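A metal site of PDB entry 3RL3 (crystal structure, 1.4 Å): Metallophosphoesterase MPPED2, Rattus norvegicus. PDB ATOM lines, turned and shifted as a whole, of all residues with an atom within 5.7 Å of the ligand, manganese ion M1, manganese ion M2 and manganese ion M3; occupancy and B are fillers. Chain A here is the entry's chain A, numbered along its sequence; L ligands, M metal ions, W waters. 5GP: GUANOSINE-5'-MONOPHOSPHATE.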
ATOM      1  N   ASP A  67     -18.054   3.426  -2.740  1.00  0.00           N
ATOM      2  CA  ASP A  67     -17.302   4.104  -1.652  1.00  0.00           C
ATOM      3  C   ASP A  67     -18.233   4.435  -0.491  1.00  0.00           C
ATOM      4  O   ASP A  67     -18.254   5.555   0.018  1.00  0.00           O
ATOM      5  CB  ASP A  67     -16.616   5.359  -2.211  1.00  0.00           C
ATOM      6  CG  ASP A  67     -15.532   4.987  -3.211  1.00  0.00           C
ATOM      7  OD1 ASP A  67     -14.386   4.736  -2.764  1.00  0.00           O
ATOM      8  OD2 ASP A  67     -15.846   4.940  -4.429  1.00  0.00           O
ATOM      9  N   HIS A  69     -17.993   2.614   2.367  1.00  0.00           N
ATOM     10  CA  HIS A  69     -17.066   2.556   3.503  1.00  0.00           C
ATOM     11  C   HIS A  69     -17.761   2.163   4.798  1.00  0.00           C
ATOM     12  O   HIS A  69     -17.445   2.694   5.863  1.00  0.00           O
ATOM     13  CB  HIS A  69     -16.307   3.880   3.626  1.00  0.00           C
ATOM     14  CG  HIS A  69     -15.264   4.072   2.568  1.00  0.00           C
ATOM     15  ND1 HIS A  69     -14.037   3.455   2.626  1.00  0.00           N
ATOM     16  CD2 HIS A  69     -15.284   4.773   1.410  1.00  0.00           C
ATOM     17  CE1 HIS A  69     -13.329   3.783   1.557  1.00  0.00           C
ATOM     18  NE2 HIS A  69     -14.061   4.585   0.794  1.00  0.00           N
ATOM     19  N   GLY A  87     -17.282  -0.415  -5.383  1.00  0.00           N
ATOM     20  CA  GLY A  87     -16.152  -0.801  -4.494  1.00  0.00           C
ATOM     21  C   GLY A  87     -15.937   0.100  -3.295  1.00  0.00           C
ATOM     22  O   GLY A  87     -16.605   1.145  -3.139  1.00  0.00           O
ATOM     23  N   ASP A  88     -14.989  -0.272  -2.437  1.00  0.00           N
ATOM     24  CA  ASP A  88     -14.827   0.364  -1.138  1.00  0.00           C
ATOM     25  C   ASP A  88     -16.153   0.303  -0.380  1.00  0.00           C
ATOM     26  O   ASP A  88     -16.667   1.323   0.128  1.00  0.00           O
ATOM     27  CB  ASP A  88     -14.320   1.819  -1.237  1.00  0.00           C
ATOM     28  CG  ASP A  88     -12.815   1.904  -1.491  1.00  0.00           C
ATOM     29  OD1 ASP A  88     -12.129   0.860  -1.576  1.00  0.00           O
ATOM     30  OD2 ASP A  88     -12.328   3.043  -1.627  1.00  0.00           O
ATOM     31  N   GLY A 118     -13.007  -2.560  -4.210  1.00  0.00           N
ATOM     32  CA  GLY A 118     -12.044  -1.484  -4.351  1.00  0.00           C
ATOM     33  C   GLY A 118     -10.797  -1.739  -3.518  1.00  0.00           C
ATOM     34  O   GLY A 118     -10.584  -2.858  -3.009  1.00  0.00           O
ATOM     35  N   ASN A 119      -9.998  -0.696  -3.349  1.00  0.00           N
ATOM     36  CA  ASN A 119      -8.701  -0.856  -2.640  1.00  0.00           C
ATOM     37  C   ASN A 119      -8.837  -1.149  -1.156  1.00  0.00           C
ATOM     38  O   ASN A 119      -7.908  -1.688  -0.546  1.00  0.00           O
ATOM     39  CB  ASN A 119      -7.772   0.328  -2.888  1.00  0.00           C
ATOM     40  CG  ASN A 119      -8.393   1.607  -2.524  1.00  0.00           C
ATOM     41  OD1 ASN A 119      -9.511   1.901  -2.932  1.00  0.00           O
ATOM     42  ND2 ASN A 119      -7.667   2.433  -1.794  1.00  0.00           N
ATOM     43  N   HIS A 120      -9.983  -0.811  -0.576  1.00  0.00           N
ATOM     44  CA  HIS A 120     -10.153  -1.094   0.855  1.00  0.00           C
ATOM     45  C   HIS A 120     -10.524  -2.552   1.144  1.00  0.00           C
ATOM     46  O   HIS A 120     -10.456  -2.979   2.305  1.00  0.00           O
ATOM     47  CB  HIS A 120     -11.159  -0.144   1.504  1.00  0.00           C
ATOM     48  CG  HIS A 120     -10.600   1.224   1.766  1.00  0.00           C
ATOM     49  ND1 HIS A 120     -10.273   1.666   3.027  1.00  0.00           N
ATOM     50  CD2 HIS A 120     -10.241   2.221   0.917  1.00  0.00           C
ATOM     51  CE1 HIS A 120      -9.790   2.893   2.956  1.00  0.00           C
ATOM     52  NE2 HIS A 120      -9.730   3.244   1.677  1.00  0.00           N
ATOM     53  N   PRO A 183      -4.642   2.510 -10.403  1.00  0.00           N
ATOM     54  CA  PRO A 183      -3.213   2.859 -10.402  1.00  0.00           C
ATOM     55  C   PRO A 183      -2.642   2.934  -8.986  1.00  0.00           C
ATOM     56  O   PRO A 183      -3.299   3.426  -8.069  1.00  0.00           O
ATOM     57  CB  PRO A 183      -3.153   4.219 -11.095  1.00  0.00           C
ATOM     58  CG  PRO A 183      -4.498   4.465 -11.728  1.00  0.00           C
ATOM     59  CD  PRO A 183      -5.488   3.527 -11.071  1.00  0.00           C
ATOM     60  N   TRP A 184      -1.424   2.419  -8.825  1.00  0.00           N
ATOM     61  CA  TRP A 184      -0.783   2.316  -7.523  1.00  0.00           C
ATOM     62  C   TRP A 184      -0.844   3.646  -6.788  1.00  0.00           C
ATOM     63  O   TRP A 184      -0.497   4.686  -7.333  1.00  0.00           O
ATOM     64  CB  TRP A 184       0.682   1.888  -7.700  1.00  0.00           C
ATOM     65  CG  TRP A 184       1.264   1.264  -6.427  1.00  0.00           C
ATOM     66  CD1 TRP A 184       1.304  -0.066  -6.125  1.00  0.00           C
ATOM     67  CD2 TRP A 184       1.876   1.949  -5.340  1.00  0.00           C
ATOM     68  NE1 TRP A 184       1.906  -0.240  -4.891  1.00  0.00           N
ATOM     69  CE2 TRP A 184       2.254   0.974  -4.391  1.00  0.00           C
ATOM     70  CE3 TRP A 184       2.150   3.298  -5.068  1.00  0.00           C
ATOM     71  CZ2 TRP A 184       2.902   1.310  -3.193  1.00  0.00           C
ATOM     72  CZ3 TRP A 184       2.790   3.629  -3.869  1.00  0.00           C
ATOM     73  CH2 TRP A 184       3.142   2.633  -2.953  1.00  0.00           C
ATOM     74  N   PHE A 185      -1.315   3.592  -5.552  1.00  0.00           N
ATOM     75  CA  PHE A 185      -1.437   4.773  -4.741  1.00  0.00           C
ATOM     76  C   PHE A 185      -0.743   4.533  -3.402  1.00  0.00           C
ATOM     77  O   PHE A 185       0.291   5.148  -3.141  1.00  0.00           O
ATOM     78  CB  PHE A 185      -2.911   5.149  -4.590  1.00  0.00           C
ATOM     79  CG  PHE A 185      -3.147   6.358  -3.747  1.00  0.00           C
ATOM     80  CD1 PHE A 185      -2.458   7.546  -3.990  1.00  0.00           C
ATOM     81  CD2 PHE A 185      -4.098   6.329  -2.737  1.00  0.00           C
ATOM     82  CE1 PHE A 185      -2.687   8.670  -3.190  1.00  0.00           C
ATOM     83  CE2 PHE A 185      -4.347   7.446  -1.943  1.00  0.00           C
ATOM     84  CZ  PHE A 185      -3.628   8.621  -2.177  1.00  0.00           C
ATOM     85  N   ASN A 186      -1.242   3.600  -2.601  1.00  0.00           N
ATOM     86  CA  ASN A 186      -0.676   3.322  -1.260  1.00  0.00           C
ATOM     87  C   ASN A 186      -0.327   1.855  -1.073  1.00  0.00           C
ATOM     88  O   ASN A 186       0.029   1.431   0.037  1.00  0.00           O
ATOM     89  CB  ASN A 186      -1.649   3.684  -0.131  1.00  0.00           C
ATOM     90  CG  ASN A 186      -2.052   5.143  -0.129  1.00  0.00           C
ATOM     91  OD1 ASN A 186      -1.223   6.043  -0.260  1.00  0.00           O
ATOM     92  ND2 ASN A 186      -3.351   5.388   0.068  1.00  0.00           N
ATOM     93  N   ARG A 194       0.913   2.033 -13.240  1.00  0.00           N
ATOM     94  CA  ARG A 194       0.434   2.503 -14.518  1.00  0.00           C
ATOM     95  C   ARG A 194       1.148   1.829 -15.679  1.00  0.00           C
ATOM     96  O   ARG A 194       2.309   1.412 -15.576  1.00  0.00           O
ATOM     97  CB  ARG A 194       0.593   4.023 -14.593  1.00  0.00           C
ATOM     98  CG  ARG A 194      -0.347   4.756 -13.653  1.00  0.00           C
ATOM     99  CD  ARG A 194      -0.193   6.285 -13.724  1.00  0.00           C
ATOM    100  NE  ARG A 194      -0.945   6.929 -12.639  1.00  0.00           N
ATOM    101  CZ  ARG A 194      -2.222   7.269 -12.722  1.00  0.00           C
ATOM    102  NH1 ARG A 194      -2.915   7.037 -13.828  1.00  0.00           N
ATOM    103  NH2 ARG A 194      -2.818   7.847 -11.673  1.00  0.00           N
ATOM    104  N   HIS A 215     -13.210   0.432 -10.109  1.00  0.00           N
ATOM    105  CA  HIS A 215     -13.243   1.149  -8.846  1.00  0.00           C
ATOM    106  C   HIS A 215     -12.899   2.613  -9.048  1.00  0.00           C
ATOM    107  O   HIS A 215     -13.491   3.482  -8.426  1.00  0.00           O
ATOM    108  CB  HIS A 215     -12.361   0.515  -7.784  1.00  0.00           C
ATOM    109  CG  HIS A 215     -12.367   1.294  -6.497  1.00  0.00           C
ATOM    110  ND1 HIS A 215     -13.544   1.601  -5.832  1.00  0.00           N
ATOM    111  CD2 HIS A 215     -11.361   1.843  -5.769  1.00  0.00           C
ATOM    112  CE1 HIS A 215     -13.258   2.320  -4.760  1.00  0.00           C
ATOM    113  NE2 HIS A 215     -11.942   2.486  -4.690  1.00  0.00           N
ATOM    114  N   VAL A 225      -8.154  15.557  -8.424  1.00  0.00           N
ATOM    115  CA  VAL A 225      -7.882  15.515  -6.983  1.00  0.00           C
ATOM    116  C   VAL A 225      -7.443  16.930  -6.561  1.00  0.00           C
ATOM    117  O   VAL A 225      -6.297  17.311  -6.807  1.00  0.00           O
ATOM    118  CB  VAL A 225      -6.813  14.440  -6.630  1.00  0.00           C
ATOM    119  CG1 VAL A 225      -6.535  14.399  -5.136  1.00  0.00           C
ATOM    120  CG2 VAL A 225      -7.265  13.060  -7.113  1.00  0.00           C
ATOM    121  N   LYS A 227      -6.606  18.443  -3.810  1.00  0.00           N
ATOM    122  CA  LYS A 227      -5.494  18.618  -2.878  1.00  0.00           C
ATOM    123  C   LYS A 227      -4.157  18.516  -3.586  1.00  0.00           C
ATOM    124  O   LYS A 227      -3.193  19.164  -3.183  1.00  0.00           O
ATOM    125  CB  LYS A 227      -5.573  17.659  -1.682  1.00  0.00           C
ATOM    126  CG  LYS A 227      -5.365  16.204  -1.987  1.00  0.00           C
ATOM    127  CD  LYS A 227      -6.030  15.336  -0.929  1.00  0.00           C
ATOM    128  CE  LYS A 227      -6.401  13.978  -1.505  1.00  0.00           C
ATOM    129  NZ  LYS A 227      -7.233  13.186  -0.570  1.00  0.00           N
ATOM    130  N   GLU A 228      -4.106  17.698  -4.647  1.00  0.00           N
ATOM    131  CA  GLU A 228      -2.870  17.480  -5.387  1.00  0.00           C
ATOM    132  C   GLU A 228      -2.771  18.323  -6.650  1.00  0.00           C
ATOM    133  O   GLU A 228      -1.700  18.379  -7.271  1.00  0.00           O
ATOM    134  CB  GLU A 228      -2.715  16.002  -5.772  1.00  0.00           C
ATOM    135  CG  GLU A 228      -2.435  15.090  -4.598  1.00  0.00           C
ATOM    136  CD  GLU A 228      -1.083  15.370  -3.974  1.00  0.00           C
ATOM    137  OE1 GLU A 228      -0.059  14.830  -4.455  1.00  0.00           O
ATOM    138  OE2 GLU A 228      -1.044  16.149  -2.996  1.00  0.00           O
ATOM    139  N   GLN A 230      -4.058  17.586  -9.477  1.00  0.00           N
ATOM    140  CA  GLN A 230      -3.666  16.589 -10.457  1.00  0.00           C
ATOM    141  C   GLN A 230      -4.869  15.780 -10.911  1.00  0.00           C
ATOM    142  O   GLN A 230      -5.802  15.519 -10.127  1.00  0.00           O
ATOM    143  CB  GLN A 230      -2.625  15.636  -9.879  1.00  0.00           C
ATOM    144  CG  GLN A 230      -1.210  16.220  -9.805  1.00  0.00           C
ATOM    145  CD  GLN A 230      -0.138  15.161  -9.656  1.00  0.00           C
ATOM    146  OE1 GLN A 230      -0.394  14.071  -9.143  1.00  0.00           O
ATOM    147  NE2 GLN A 230       1.071  15.488 -10.103  1.00  0.00           N
ATOM    148  N   VAL A 232      -5.875  11.987 -11.959  1.00  0.00           N
ATOM    149  CA  VAL A 232      -5.294  10.707 -11.556  1.00  0.00           C
ATOM    150  C   VAL A 232      -5.923   9.489 -12.250  1.00  0.00           C
ATOM    151  O   VAL A 232      -5.571   8.346 -11.932  1.00  0.00           O
ATOM    152  CB  VAL A 232      -5.340  10.491 -10.017  1.00  0.00           C
ATOM    153  CG1 VAL A 232      -4.593  11.622  -9.277  1.00  0.00           C
ATOM    154  CG2 VAL A 232      -6.776  10.392  -9.514  1.00  0.00           C
ATOM    155  N   GLY A 254     -13.881   5.835  -6.425  1.00  0.00           N
ATOM    156  CA  GLY A 254     -12.432   5.928  -6.221  1.00  0.00           C
ATOM    157  C   GLY A 254     -12.009   7.297  -5.745  1.00  0.00           C
ATOM    158  O   GLY A 254     -11.499   7.448  -4.625  1.00  0.00           O
ATOM    159  N   ILE A 255     -12.212   8.279  -6.611  1.00  0.00           N
ATOM    160  CA  ILE A 255     -11.938   9.688  -6.264  1.00  0.00           C
ATOM    161  C   ILE A 255     -13.227  10.287  -5.740  1.00  0.00           C
ATOM    162  O   ILE A 255     -14.114  10.666  -6.526  1.00  0.00           O
ATOM    163  CB  ILE A 255     -11.378  10.440  -7.484  1.00  0.00           C
ATOM    164  CG1 ILE A 255     -10.116   9.720  -8.008  1.00  0.00           C
ATOM    165  CG2 ILE A 255     -11.072  11.917  -7.145  1.00  0.00           C
ATOM    166  CD1 ILE A 255      -9.003   9.469  -6.937  1.00  0.00           C
ATOM    167  N   HIS A 256     -13.362  10.325  -4.417  1.00  0.00           N
ATOM    168  CA  HIS A 256     -14.651  10.726  -3.808  1.00  0.00           C
ATOM    169  C   HIS A 256     -15.057  12.116  -4.267  1.00  0.00           C
ATOM    170  O   HIS A 256     -16.254  12.377  -4.510  1.00  0.00           O
ATOM    171  CB  HIS A 256     -14.583  10.702  -2.280  1.00  0.00           C
ATOM    172  CG  HIS A 256     -14.299   9.357  -1.682  1.00  0.00           C
ATOM    173  ND1 HIS A 256     -14.291   9.154  -0.318  1.00  0.00           N
ATOM    174  CD2 HIS A 256     -14.007   8.145  -2.235  1.00  0.00           C
ATOM    175  CE1 HIS A 256     -13.989   7.901  -0.045  1.00  0.00           C
ATOM    176  NE2 HIS A 256     -13.811   7.256  -1.193  1.00  0.00           N
ATOM    177  N   GLU A 257     -14.063  12.987  -4.378  1.00  0.00           N
ATOM    178  CA  GLU A 257     -14.261  14.399  -4.803  1.00  0.00           C
ATOM    179  C   GLU A 257     -14.907  14.541  -6.167  1.00  0.00           C
ATOM    180  O   GLU A 257     -15.448  15.608  -6.511  1.00  0.00           O
ATOM    181  CB  GLU A 257     -12.916  15.158  -4.835  1.00  0.00           C
ATOM    182  CG  GLU A 257     -12.108  15.161  -3.567  1.00  0.00           C
ATOM    183  CD  GLU A 257     -11.119  14.021  -3.531  1.00  0.00           C
ATOM    184  OE1 GLU A 257     -11.568  12.870  -3.509  1.00  0.00           O
ATOM    185  OE2 GLU A 257      -9.892  14.225  -3.477  1.00  0.00           O
ATOM    186  N   VAL A 277     -14.788  13.335   0.476  1.00  0.00           N
ATOM    187  CA  VAL A 277     -13.361  13.122   0.768  1.00  0.00           C
ATOM    188  C   VAL A 277     -13.105  13.020   2.292  1.00  0.00           C
ATOM    189  O   VAL A 277     -12.086  12.466   2.717  1.00  0.00           O
ATOM    190  CB  VAL A 277     -12.471  14.225   0.098  1.00  0.00           C
ATOM    191  CG1 VAL A 277     -12.697  15.576   0.778  1.00  0.00           C
ATOM    192  CG2 VAL A 277     -10.981  13.811   0.116  1.00  0.00           C
ATOM    193  N   PHE A 279     -15.211  11.354   4.174  1.00  0.00           N
ATOM    194  CA  PHE A 279     -15.848  10.086   4.506  1.00  0.00           C
ATOM    195  C   PHE A 279     -17.253  10.227   5.093  1.00  0.00           C
ATOM    196  O   PHE A 279     -17.701   9.386   5.878  1.00  0.00           O
ATOM    197  CB  PHE A 279     -14.917   9.208   5.372  1.00  0.00           C
ATOM    198  CG  PHE A 279     -13.807   8.548   4.573  1.00  0.00           C
ATOM    199  CD1 PHE A 279     -12.726   9.289   4.118  1.00  0.00           C
ATOM    200  CD2 PHE A 279     -13.864   7.186   4.266  1.00  0.00           C
ATOM    201  CE1 PHE A 279     -11.698   8.664   3.365  1.00  0.00           C
ATOM    202  CE2 PHE A 279     -12.850   6.570   3.532  1.00  0.00           C
ATOM    203  CZ  PHE A 279     -11.768   7.311   3.077  1.00  0.00           C
HETATM  204  P   5GP L   1      -9.819   5.615  -0.697  1.00  0.00           P
HETATM  205  O1P 5GP L   1      -9.514   4.631  -1.790  1.00  0.00           O
HETATM  206  O2P 5GP L   1     -11.301   5.491  -0.113  1.00  0.00           O
HETATM  207  O3P 5GP L   1      -8.797   5.428   0.476  1.00  0.00           O
HETATM  208  O5' 5GP L   1      -9.633   7.104  -1.284  1.00  0.00           O
HETATM  209  C5' 5GP L   1     -10.077   8.237  -0.538  1.00  0.00           C
HETATM  210  C4' 5GP L   1      -9.487   9.526  -1.189  1.00  0.00           C
HETATM  211  O4' 5GP L   1      -8.050   9.346  -1.360  1.00  0.00           O
HETATM  212  C3' 5GP L   1      -9.935   9.841  -2.617  1.00  0.00           C
HETATM  213  O3' 5GP L   1     -11.180  10.490  -2.582  1.00  0.00           O
HETATM  214  C2' 5GP L   1      -8.826  10.788  -3.075  1.00  0.00           C
HETATM  215  O2' 5GP L   1      -8.892  12.072  -2.398  1.00  0.00           O
HETATM  216  C1' 5GP L   1      -7.616  10.044  -2.541  1.00  0.00           C
HETATM  217  N9  5GP L   1      -7.136   9.125  -3.596  1.00  0.00           N
HETATM  218  C8  5GP L   1      -7.603   7.914  -3.918  1.00  0.00           C
HETATM  219  N7  5GP L   1      -6.891   7.425  -4.938  1.00  0.00           N
HETATM  220  C5  5GP L   1      -5.973   8.329  -5.268  1.00  0.00           C
HETATM  221  C6  5GP L   1      -4.970   8.399  -6.236  1.00  0.00           C
HETATM  222  O6  5GP L   1      -4.769   7.465  -7.008  1.00  0.00           O
HETATM  223  N1  5GP L   1      -4.166   9.533  -6.301  1.00  0.00           N
HETATM  224  C2  5GP L   1      -4.390  10.584  -5.395  1.00  0.00           C
HETATM  225  N2  5GP L   1      -3.627  11.672  -5.431  1.00  0.00           N
HETATM  226  N3  5GP L   1      -5.366  10.495  -4.485  1.00  0.00           N
HETATM  227  C4  5GP L   1      -6.139   9.409  -4.413  1.00  0.00           C
HETATM  228 MN    MN M   1     -13.087   5.108  -1.150  1.00  0.00          MN
HETATM  229 MN    MN M   2     -10.700   3.559  -3.138  1.00  0.00          MN
HETATM  230 MN    MN M   3      -7.021   6.231   1.255  1.00  0.00          MN
HETATM  231  O   HOH W   1      -5.481   4.724  -7.169  1.00  0.00           O
HETATM  232  O   HOH W   2      -2.195   6.852  -8.500  1.00  0.00           O
HETATM  233  O   HOH W   3      -9.348   4.095  -4.685  1.00  0.00           O
HETATM  234  O   HOH W   4      -5.383  10.396   0.439  1.00  0.00           O
HETATM  235  O   HOH W   5      -7.873   6.943   2.578  1.00  0.00           O
HETATM  236  O   HOH W   6     -11.925   5.346  -3.170  1.00  0.00           O
HETATM  237  O   HOH W   7      -9.145   5.889  -6.749  1.00  0.00           O
HETATM  238  O   HOH W   8      -6.100   4.190   0.411  1.00  0.00           O
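Manganese ion M3 is bound by water W5 (1.7 Å). Manganese ion M3 is bound by an oxygen (O3P) of the ligand. Water W8 binds manganese ion M3 (2.4 Å).
N of Gly 254 lies within hydrogen-bond range of OD2 of Asp 67 (2.9 Å). The backbone NH (N) of Asp 67 is in hydrogen-bond range of the backbone carbonyl oxygen (O) of Gly 87 (2.7 Å). The backbone NH (N) of His 120 is in hydrogen-bond range of the side-chain carboxylate (OD1) of Asp 88, 2.9 Å away. The backbone carbonyl oxygen (O) of His 215 sits at hydrogen-bond distance from the backbone NH (N) of Gly 254 (3.1 Å). The backbone carbonyl oxygen of Val 232 is in hydrogen-bond range of the guanidinium group of Arg 194 (2.8 Å). The backbone carbonyl oxygen (O) of Gln 230 sits at hydrogen-bond distance from the backbone NH (N) of Val 225 (2.9 Å).
Merely in contact with manganese ion M3: Asn 186. Of the 24 residues printed, 1 comes within 4 Å of manganese ion M3. The nearest printed residue that does not touch manganese ion M3 is His 120 (4.1 Å).
Within 4 Å of manganese ion M1: Asp 67, His 69, Asp 88 and His 256.
Manganese ion M1 is bound by O2P of the ligand (2.1 Å), OD1 of Asp 67 (2.1 Å), NE2 of His 69 (2.2 Å), OD2 of Asp 88 (2.3 Å), NE2 of His 256 (2.3 Å) and water W6 (2.3 Å).
Water W6 bridges the backbone carbonyl oxygen (O) of Gly 254 (2.6 Å) and an oxygen (O5') of the ligand (3.4 Å). Water W8 bridges the side-chain amide nitrogen (ND2) of Asn 186 (3.0 Å) and the side-chain amide nitrogen (ND2) of Asn 119 (3.2 Å). Water W1 bridges the backbone carbonyl oxygen of Pro 183 and an oxygen (O6) of the ligand. Water W2 lies within hydrogen-bond range of the backbone carbonyl oxygen of Trp 184 (3.0 Å), an oxygen (O6) of the ligand (3.0 Å) and the guanidinium group of Arg 194 (3.4 Å). Water W4 bridges O4' of the ligand (3.4 Å) and NZ of Lys 227 (3.5 Å).
The backbone NH (N) of His 256 sits at hydrogen-bond distance from an oxygen (O3') of the ligand (2.9 Å). The side-chain carboxylate (OE1) of Glu 257 is in hydrogen-bond range of an oxygen (O3') of the ligand (2.6 Å). An oxygen (O3P) of the ligand sits close to a ring nitrogen (NE2) of His 120. An oxygen (O2') of the ligand sits at hydrogen-bond distance from the side-chain amino group (NZ) of Lys 227 (2.7 Å).
Phe 185 touches the ligand (CE1 to C2, 3.4 Å). CG1 of Val 225 touches N2 of the ligand, 3.998 Å away. Glu 228 touches the ligand. Val 232 touches the ligand. Gly 254 touches the ligand (O to C3', 3.5 Å). Ile 255 touches the ligand (CD1 to N7, 3.6 Å). CG2 of Val 277 touches O2' of the ligand, at 3.7 Å. Phe 279 touches the ligand (CZ to O2P, 3.7 Å). Within 4 Å of the ligand: His 69, Asp 88, Asn 119, His 120, Phe 185, Val 225, Lys 227, Glu 228, Val 232, Gly 254, Ile 255, His 256, Glu 257, Val 277 and Phe 279.
Manganese ion M2 is bound by the side-chain amide oxygen (OD1) of Asn 119. O1P of the ligand binds manganese ion M2, 2.1 Å away. Manganese ion M2 is bound by water W3 (2.1 Å). Water W6 binds manganese ion M2, 2.2 Å away. Manganese ion M2 is bound by NE2 of His 215, 2.3 Å away. OD2 of Asp 88 is bound to manganese ion M2 (2.3 Å).
Of the 24 residues printed, 4 come within 4 Å of manganese ion M2. The nearest printed residue that does not touch manganese ion M2 is Gly 254 (4.2 Å).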
